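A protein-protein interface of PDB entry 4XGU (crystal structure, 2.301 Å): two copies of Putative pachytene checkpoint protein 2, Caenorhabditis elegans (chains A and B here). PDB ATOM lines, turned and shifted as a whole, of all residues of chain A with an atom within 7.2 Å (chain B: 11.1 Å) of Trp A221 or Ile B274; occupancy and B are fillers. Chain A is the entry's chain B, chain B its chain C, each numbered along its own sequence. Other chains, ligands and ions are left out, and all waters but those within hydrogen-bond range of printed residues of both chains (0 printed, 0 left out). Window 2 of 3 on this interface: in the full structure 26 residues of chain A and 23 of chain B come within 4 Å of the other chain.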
ATOM      1  N   SER A 216     -23.907 -20.669  11.897  1.00  0.00           N
ATOM      2  CA  SER A 216     -23.350 -20.693  10.542  1.00  0.00           C
ATOM      3  C   SER A 216     -22.460 -19.486  10.240  1.00  0.00           C
ATOM      4  O   SER A 216     -22.141 -19.220   9.081  1.00  0.00           O
ATOM      5  CB  SER A 216     -24.468 -20.781   9.497  1.00  0.00           C
ATOM      6  OG  SER A 216     -25.017 -22.086   9.445  1.00  0.00           O
ATOM      7  N   LEU A 217     -22.054 -18.762  11.280  1.00  0.00           N
ATOM      8  CA  LEU A 217     -21.151 -17.630  11.105  1.00  0.00           C
ATOM      9  C   LEU A 217     -19.759 -18.144  10.766  1.00  0.00           C
ATOM     10  O   LEU A 217     -19.051 -17.574   9.936  1.00  0.00           O
ATOM     11  CB  LEU A 217     -21.097 -16.763  12.365  1.00  0.00           C
ATOM     12  CG  LEU A 217     -22.395 -16.503  13.134  1.00  0.00           C
ATOM     13  CD1 LEU A 217     -22.132 -15.587  14.323  1.00  0.00           C
ATOM     14  CD2 LEU A 217     -23.462 -15.920  12.227  1.00  0.00           C
ATOM     15  N   PHE A 218     -19.382 -19.236  11.422  1.00  0.00           N
ATOM     16  CA  PHE A 218     -18.063 -19.830  11.267  1.00  0.00           C
ATOM     17  C   PHE A 218     -17.940 -20.598   9.952  1.00  0.00           C
ATOM     18  O   PHE A 218     -16.855 -20.696   9.384  1.00  0.00           O
ATOM     19  CB  PHE A 218     -17.770 -20.753  12.455  1.00  0.00           C
ATOM     20  CG  PHE A 218     -16.336 -21.197  12.551  1.00  0.00           C
ATOM     21  CD1 PHE A 218     -15.332 -20.286  12.840  1.00  0.00           C
ATOM     22  CD2 PHE A 218     -15.994 -22.527  12.375  1.00  0.00           C
ATOM     23  CE1 PHE A 218     -14.013 -20.691  12.936  1.00  0.00           C
ATOM     24  CE2 PHE A 218     -14.677 -22.940  12.470  1.00  0.00           C
ATOM     25  CZ  PHE A 218     -13.686 -22.019  12.752  1.00  0.00           C
ATOM     26  N   SER A 219     -19.066 -21.117   9.467  1.00  0.00           N
ATOM     27  CA  SER A 219     -19.086 -22.026   8.321  1.00  0.00           C
ATOM     28  C   SER A 219     -18.566 -21.417   7.017  1.00  0.00           C
ATOM     29  O   SER A 219     -17.799 -22.056   6.297  1.00  0.00           O
ATOM     30  CB  SER A 219     -20.506 -22.554   8.101  1.00  0.00           C
ATOM     31  OG  SER A 219     -21.405 -21.498   7.813  1.00  0.00           O
ATOM     32  N   LYS A 220     -18.989 -20.193   6.708  1.00  0.00           N
ATOM     33  CA  LYS A 220     -18.596 -19.539   5.460  1.00  0.00           C
ATOM     34  C   LYS A 220     -17.092 -19.291   5.387  1.00  0.00           C
ATOM     35  O   LYS A 220     -16.464 -19.528   4.353  1.00  0.00           O
ATOM     36  CB  LYS A 220     -19.349 -18.219   5.286  1.00  0.00           C
ATOM     37  CG  LYS A 220     -20.657 -18.353   4.517  1.00  0.00           C
ATOM     38  CD  LYS A 220     -20.410 -18.732   3.061  1.00  0.00           C
ATOM     39  CE  LYS A 220     -20.356 -17.509   2.151  1.00  0.00           C
ATOM     40  NZ  LYS A 220     -19.249 -16.572   2.493  1.00  0.00           N
ATOM     41  N   TRP A 221     -16.519 -18.812   6.488  1.00  0.00           N
ATOM     42  CA  TRP A 221     -15.075 -18.632   6.582  1.00  0.00           C
ATOM     43  C   TRP A 221     -14.381 -19.990   6.637  1.00  0.00           C
ATOM     44  O   TRP A 221     -13.235 -20.137   6.209  1.00  0.00           O
ATOM     45  CB  TRP A 221     -14.714 -17.797   7.811  1.00  0.00           C
ATOM     46  N   PHE A 222     -15.094 -20.979   7.169  1.00  0.00           N
ATOM     47  CA  PHE A 222     -14.602 -22.350   7.236  1.00  0.00           C
ATOM     48  C   PHE A 222     -14.653 -23.006   5.859  1.00  0.00           C
ATOM     49  O   PHE A 222     -13.766 -23.779   5.497  1.00  0.00           O
ATOM     50  CB  PHE A 222     -15.418 -23.158   8.247  1.00  0.00           C
ATOM     51  CG  PHE A 222     -15.033 -24.603   8.329  1.00  0.00           C
ATOM     52  CD1 PHE A 222     -14.000 -25.012   9.154  1.00  0.00           C
ATOM     53  CD2 PHE A 222     -15.717 -25.556   7.591  1.00  0.00           C
ATOM     54  CE1 PHE A 222     -13.650 -26.342   9.233  1.00  0.00           C
ATOM     55  CE2 PHE A 222     -15.372 -26.885   7.666  1.00  0.00           C
ATOM     56  CZ  PHE A 222     -14.337 -27.280   8.488  1.00  0.00           C
ATOM     57  N   SER A 223     -15.700 -22.698   5.098  1.00  0.00           N
ATOM     58  CA  SER A 223     -15.814 -23.171   3.723  1.00  0.00           C
ATOM     59  C   SER A 223     -14.729 -22.519   2.865  1.00  0.00           C
ATOM     60  O   SER A 223     -14.101 -23.175   2.032  1.00  0.00           O
ATOM     61  CB  SER A 223     -17.209 -22.875   3.163  1.00  0.00           C
ATOM     62  OG  SER A 223     -18.212 -23.551   3.907  1.00  0.00           O
ATOM     63  N   GLU A 224     -14.512 -21.224   3.087  1.00  0.00           N
ATOM     64  CA  GLU A 224     -13.382 -20.513   2.492  1.00  0.00           C
ATOM     65  C   GLU A 224     -12.071 -21.135   2.962  1.00  0.00           C
ATOM     66  O   GLU A 224     -11.072 -21.122   2.238  1.00  0.00           O
ATOM     67  CB  GLU A 224     -13.415 -19.028   2.861  1.00  0.00           C
ATOM     68  CG  GLU A 224     -12.284 -18.204   2.247  1.00  0.00           C
ATOM     69  CD  GLU A 224     -11.664 -17.230   3.234  1.00  0.00           C
ATOM     70  OE1 GLU A 224     -10.779 -17.651   4.008  1.00  0.00           O
ATOM     71  OE2 GLU A 224     -12.068 -16.049   3.245  1.00  0.00           O
ATOM     72  N   SER A 225     -12.103 -21.658   4.190  1.00  0.00           N
ATOM     73  CA  SER A 225     -10.969 -22.293   4.879  1.00  0.00           C
ATOM     74  C   SER A 225      -9.991 -21.273   5.461  1.00  0.00           C
ATOM     75  O   SER A 225      -9.789 -20.191   4.908  1.00  0.00           O
ATOM     76  CB  SER A 225     -10.214 -23.257   3.957  1.00  0.00           C
ATOM     77  OG  SER A 225     -11.099 -24.161   3.322  1.00  0.00           O
ATOM     78  N   GLY A 226      -9.387 -21.637   6.585  1.00  0.00           N
ATOM     79  CA  GLY A 226      -8.429 -20.788   7.263  1.00  0.00           C
ATOM     80  C   GLY A 226      -7.558 -21.577   8.223  1.00  0.00           C
ATOM     81  O   GLY A 226      -7.856 -22.729   8.534  1.00  0.00           O
ATOM     82  N   LEU A 228      -6.939 -20.600  11.304  1.00  0.00           N
ATOM     83  CA  LEU A 228      -7.312 -20.252  12.670  1.00  0.00           C
ATOM     84  C   LEU A 228      -8.265 -21.241  13.338  1.00  0.00           C
ATOM     85  O   LEU A 228      -8.591 -21.081  14.513  1.00  0.00           O
ATOM     86  CB  LEU A 228      -7.925 -18.853  12.695  1.00  0.00           C
ATOM     87  CG  LEU A 228      -8.964 -18.562  11.615  1.00  0.00           C
ATOM     88  CD1 LEU A 228     -10.328 -18.320  12.236  1.00  0.00           C
ATOM     89  CD2 LEU A 228      -8.523 -17.370  10.778  1.00  0.00           C
ATOM     90  N   VAL A 229      -8.716 -22.252  12.603  1.00  0.00           N
ATOM     91  CA  VAL A 229      -9.432 -23.351  13.237  1.00  0.00           C
ATOM     92  C   VAL A 229      -8.468 -24.013  14.213  1.00  0.00           C
ATOM     93  O   VAL A 229      -8.836 -24.358  15.334  1.00  0.00           O
ATOM     94  CB  VAL A 229      -9.958 -24.381  12.221  1.00  0.00           C
ATOM     95  CG1 VAL A 229     -10.633 -25.541  12.941  1.00  0.00           C
ATOM     96  CG2 VAL A 229     -10.919 -23.723  11.244  1.00  0.00           C
ATOM     97  N   LEU A 257     -20.426 -26.942   8.064  1.00  0.00           N
ATOM     98  CA  LEU A 257     -18.971 -27.027   8.056  1.00  0.00           C
ATOM     99  C   LEU A 257     -18.519 -28.153   7.130  1.00  0.00           C
ATOM    100  O   LEU A 257     -17.855 -27.916   6.120  1.00  0.00           O
ATOM    101  CB  LEU A 257     -18.433 -27.260   9.472  1.00  0.00           C
ATOM    102  CG  LEU A 257     -18.764 -26.204  10.529  1.00  0.00           C
ATOM    103  CD1 LEU A 257     -18.459 -26.724  11.926  1.00  0.00           C
ATOM    104  CD2 LEU A 257     -17.995 -24.925  10.261  1.00  0.00           C
ATOM    105  N   ALA A 276      -9.936 -27.704   5.590  1.00  0.00           N
ATOM    106  CA  ALA A 276     -10.153 -27.304   6.976  1.00  0.00           C
ATOM    107  C   ALA A 276     -10.938 -28.346   7.773  1.00  0.00           C
ATOM    108  O   ALA A 276     -10.778 -28.447   8.990  1.00  0.00           O
ATOM    109  CB  ALA A 276     -10.868 -25.960   7.028  1.00  0.00           C
ATOM    110  N   SER B 219     -19.337  -0.242   6.320  1.00  0.00           N
ATOM    111  CA  SER B 219     -18.505  -1.272   5.708  1.00  0.00           C
ATOM    112  C   SER B 219     -17.399  -0.632   4.872  1.00  0.00           C
ATOM    113  O   SER B 219     -16.233  -1.026   4.957  1.00  0.00           O
ATOM    114  CB  SER B 219     -19.354  -2.218   4.849  1.00  0.00           C
ATOM    115  OG  SER B 219     -19.834  -1.576   3.681  1.00  0.00           O
ATOM    116  N   PHE B 222     -13.634   1.252   6.152  1.00  0.00           N
ATOM    117  CA  PHE B 222     -12.317   0.640   6.013  1.00  0.00           C
ATOM    118  C   PHE B 222     -12.347  -0.289   4.807  1.00  0.00           C
ATOM    119  O   PHE B 222     -11.486  -0.228   3.933  1.00  0.00           O
ATOM    120  CB  PHE B 222     -11.914  -0.128   7.278  1.00  0.00           C
ATOM    121  N   GLY B 226     -15.675  -2.467  12.472  1.00  0.00           N
ATOM    122  CA  GLY B 226     -14.456  -1.862  12.969  1.00  0.00           C
ATOM    123  C   GLY B 226     -14.377  -1.867  14.483  1.00  0.00           C
ATOM    124  O   GLY B 226     -15.095  -2.611  15.151  1.00  0.00           O
ATOM    125  N   VAL B 229     -17.733  -0.155  16.278  1.00  0.00           N
ATOM    126  CA  VAL B 229     -19.000  -0.860  16.446  1.00  0.00           C
ATOM    127  C   VAL B 229     -19.100  -1.461  17.845  1.00  0.00           C
ATOM    128  O   VAL B 229     -20.177  -1.504  18.429  1.00  0.00           O
ATOM    129  CB  VAL B 229     -19.207  -1.968  15.378  1.00  0.00           C
ATOM    130  CG1 VAL B 229     -19.146  -1.373  13.981  1.00  0.00           C
ATOM    131  CG2 VAL B 229     -18.193  -3.092  15.529  1.00  0.00           C
ATOM    132  N   ILE B 274     -15.004 -10.427   7.134  1.00  0.00           N
ATOM    133  CA  ILE B 274     -15.835 -11.425   7.795  1.00  0.00           C
ATOM    134  C   ILE B 274     -15.850 -11.225   9.305  1.00  0.00           C
ATOM    135  O   ILE B 274     -16.801 -11.618   9.980  1.00  0.00           O
ATOM    136  CB  ILE B 274     -15.355 -12.860   7.484  1.00  0.00           C
ATOM    137  CG1 ILE B 274     -13.888 -13.037   7.892  1.00  0.00           C
ATOM    138  CG2 ILE B 274     -15.548 -13.177   6.007  1.00  0.00           C
ATOM    139  CD1 ILE B 274     -13.325 -14.417   7.602  1.00  0.00           C
ATOM    140  N   ARG B 275     -14.797 -10.608   9.829  1.00  0.00           N
ATOM    141  CA  ARG B 275     -14.653 -10.430  11.269  1.00  0.00           C
ATOM    142  C   ARG B 275     -15.567  -9.328  11.794  1.00  0.00           C
ATOM    143  O   ARG B 275     -16.066  -9.407  12.917  1.00  0.00           O
ATOM    144  CB  ARG B 275     -13.195 -10.123  11.627  1.00  0.00           C
ATOM    145  CG  ARG B 275     -12.948  -9.951  13.118  1.00  0.00           C
ATOM    146  CD  ARG B 275     -11.499 -10.229  13.484  1.00  0.00           C
ATOM    147  NE  ARG B 275     -11.274 -10.128  14.923  1.00  0.00           N
ATOM    148  CZ  ARG B 275     -11.563 -11.087  15.796  1.00  0.00           C
ATOM    149  NH1 ARG B 275     -12.097 -12.229  15.379  1.00  0.00           N
ATOM    150  NH2 ARG B 275     -11.321 -10.907  17.087  1.00  0.00           N
ATOM    151  N   ALA B 276     -15.784  -8.304  10.975  1.00  0.00           N
ATOM    152  CA  ALA B 276     -16.623  -7.179  11.370  1.00  0.00           C
ATOM    153  C   ALA B 276     -18.084  -7.599  11.520  1.00  0.00           C
ATOM    154  O   ALA B 276     -18.772  -7.162  12.444  1.00  0.00           O
ATOM    155  CB  ALA B 276     -16.496  -6.048  10.361  1.00  0.00           C
ATOM    156  N   VAL B 277     -18.546  -8.452  10.610  1.00  0.00           N
ATOM    157  CA  VAL B 277     -19.926  -8.933  10.621  1.00  0.00           C
ATOM    158  C   VAL B 277     -20.234  -9.744  11.876  1.00  0.00           C
ATOM    159  O   VAL B 277     -21.257  -9.530  12.529  1.00  0.00           O
ATOM    160  CB  VAL B 277     -20.230  -9.800   9.384  1.00  0.00           C
ATOM    161  CG1 VAL B 277     -21.643 -10.360   9.459  1.00  0.00           C
ATOM    162  CG2 VAL B 277     -20.040  -8.990   8.113  1.00  0.00           C
ATOM    163  N   ASN B 278     -19.343 -10.677  12.198  1.00  0.00           N
ATOM    164  CA  ASN B 278     -19.470 -11.493  13.398  1.00  0.00           C
ATOM    165  C   ASN B 278     -19.585 -10.628  14.647  1.00  0.00           C
ATOM    166  O   ASN B 278     -20.481 -10.822  15.470  1.00  0.00           O
ATOM    167  CB  ASN B 278     -18.273 -12.440  13.516  1.00  0.00           C
ATOM    168  CG  ASN B 278     -18.039 -13.239  12.247  1.00  0.00           C
ATOM    169  OD1 ASN B 278     -18.979 -13.760  11.645  1.00  0.00           O
ATOM    170  ND2 ASN B 278     -16.782 -13.326  11.825  1.00  0.00           N
ATOM    171  N   ALA B 279     -18.677  -9.662  14.767  1.00  0.00           N
ATOM    172  CA  ALA B 279     -18.679  -8.721  15.881  1.00  0.00           C
ATOM    173  C   ALA B 279     -19.995  -7.951  15.951  1.00  0.00           C
ATOM    174  O   ALA B 279     -20.520  -7.697  17.037  1.00  0.00           O
ATOM    175  CB  ALA B 279     -17.505  -7.761  15.764  1.00  0.00           C
ATOM    176  N   LEU B 280     -20.527  -7.588  14.788  1.00  0.00           N
ATOM    177  CA  LEU B 280     -21.813  -6.902  14.718  1.00  0.00           C
ATOM    178  C   LEU B 280     -22.940  -7.804  15.210  1.00  0.00           C
ATOM    179  O   LEU B 280     -23.795  -7.375  15.986  1.00  0.00           O
ATOM    180  CB  LEU B 280     -22.103  -6.433  13.291  1.00  0.00           C
ATOM    181  CG  LEU B 280     -23.482  -5.812  13.051  1.00  0.00           C
ATOM    182  CD1 LEU B 280     -23.730  -4.653  14.001  1.00  0.00           C
ATOM    183  CD2 LEU B 280     -23.623  -5.356  11.607  1.00  0.00           C
ATOM    184  N   LEU B 281     -22.934  -9.054  14.760  1.00  0.00           N
ATOM    185  CA  LEU B 281     -23.957 -10.014  15.163  1.00  0.00           C
ATOM    186  C   LEU B 281     -23.865 -10.360  16.650  1.00  0.00           C
ATOM    187  O   LEU B 281     -24.889 -10.551  17.306  1.00  0.00           O
ATOM    188  CB  LEU B 281     -23.861 -11.285  14.315  1.00  0.00           C
ATOM    189  CG  LEU B 281     -24.365 -11.171  12.873  1.00  0.00           C
ATOM    190  CD1 LEU B 281     -24.138 -12.465  12.121  1.00  0.00           C
ATOM    191  CD2 LEU B 281     -25.837 -10.791  12.845  1.00  0.00           C
ATOM    192  N   THR B 282     -22.647 -10.438  17.182  1.00  0.00           N
ATOM    193  CA  THR B 282     -22.464 -10.727  18.602  1.00  0.00           C
ATOM    194  C   THR B 282     -23.041  -9.618  19.477  1.00  0.00           C
ATOM    195  O   THR B 282     -23.708  -9.889  20.477  1.00  0.00           O
ATOM    196  CB  THR B 282     -20.980 -10.919  18.966  1.00  0.00           C
ATOM    197  OG1 THR B 282     -20.219  -9.801  18.492  1.00  0.00           O
ATOM    198  CG2 THR B 282     -20.440 -12.198  18.351  1.00  0.00           C
ATOM    199  N   LYS B 307     -29.769 -16.715   6.049  1.00  0.00           N
ATOM    200  CA  LYS B 307     -29.348 -17.580   7.153  1.00  0.00           C
ATOM    201  C   LYS B 307     -29.107 -16.877   8.496  1.00  0.00           C
ATOM    202  O   LYS B 307     -29.621 -17.314   9.527  1.00  0.00           O
ATOM    203  CB  LYS B 307     -28.082 -18.350   6.762  1.00  0.00           C
ATOM    204  CG  LYS B 307     -26.944 -17.494   6.220  1.00  0.00           C
ATOM    205  CD  LYS B 307     -25.612 -18.217   6.340  1.00  0.00           C
ATOM    206  CE  LYS B 307     -25.662 -19.582   5.673  1.00  0.00           C
ATOM    207  NZ  LYS B 307     -24.414 -20.357   5.904  1.00  0.00           N
ATOM    208  N   ALA B 308     -28.347 -15.789   8.480  1.00  0.00           N
ATOM    209  CA  ALA B 308     -27.873 -15.171   9.715  1.00  0.00           C
ATOM    210  C   ALA B 308     -28.986 -14.510  10.516  1.00  0.00           C
ATOM    211  O   ALA B 308     -29.099 -14.721  11.727  1.00  0.00           O
ATOM    212  CB  ALA B 308     -26.787 -14.154   9.400  1.00  0.00           C
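The side-chain hydroxyl of Ser A223 sits at hydrogen-bond distance from the backbone carbonyl oxygen of Ser A219, 2.8 Å away.
The backbone carbonyl oxygen (O) of Asn B278 lies close to the side-chain hydroxyl (OG1) of Thr B282, 3.2 Å away.
O of Ile B274 sits at hydrogen-bond distance from ND2 of Asn B278 (2.5 Å).
The backbone carbonyl oxygen (O) of Ser A216 sits at hydrogen-bond distance from the side-chain hydroxyl (OG) of Ser A219 (2.7 Å).
NZ of Lys B307 touches CB of Ser A216, 3.6 Å away.
OD1 of Asn B278 touches CB of Leu A217, 3.7 Å away.
Leu B281 touches Leu A217 (CD1 to CD2, 3.5 Å).
Lys B307 touches Ser A219 (NZ to OG, 3.7 Å).
Ile B274 touches Trp A221 (CD1 to CB, 3.7 Å).
No residue of chain B comes within 4 Å of Phe A218.
Of chain B, only Lys B307 (3.7 Å) comes within 4 Å of Ser A219.
No residue of chain B comes within 4 Å of Lys A220.
Trp A221 touches just one residue of chain B: Ile B274.
No residue of chain B comes within 4 Å of Ser A223.
Gly A226 touches none of the printed residues of chain B.
Ala A276 touches none of the printed residues of chain B.
Ile B274 touches just one residue of chain A: Trp A221 (3.7 Å).
Printed residues of chain A within 4 Å of Asn B278: Leu A217 (3.7 Å).
Of the printed residues of chain A, Leu B281 touches Leu A217.
Ala B308 touches none of the printed residues of chain A.
The nearest residue of chain A that does not touch Ile B274 is Glu A224 (4.8 Å).
The nearest printed residue of chain A that does not touch Lys B307 is Lys A220 (4.5 Å).
Printed residues of chain A that touch a printed residue of chain B: Ser A216, Leu A217, Ser A219 and Trp A221.
Of the 15 printed residues of chain B, 4 touch a printed residue of chain A.
Hydrophobic or aromatic side chains of chain B that line the printed part of chain A: Ile B274 and Leu B281.
Among the printed residues, no Asp or Glu carboxylate lies within 4 Å of a Lys or Arg side-chain nitrogen of the other chain.
Positions printed for both chains: 219, 222, 226, 229 and 276.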
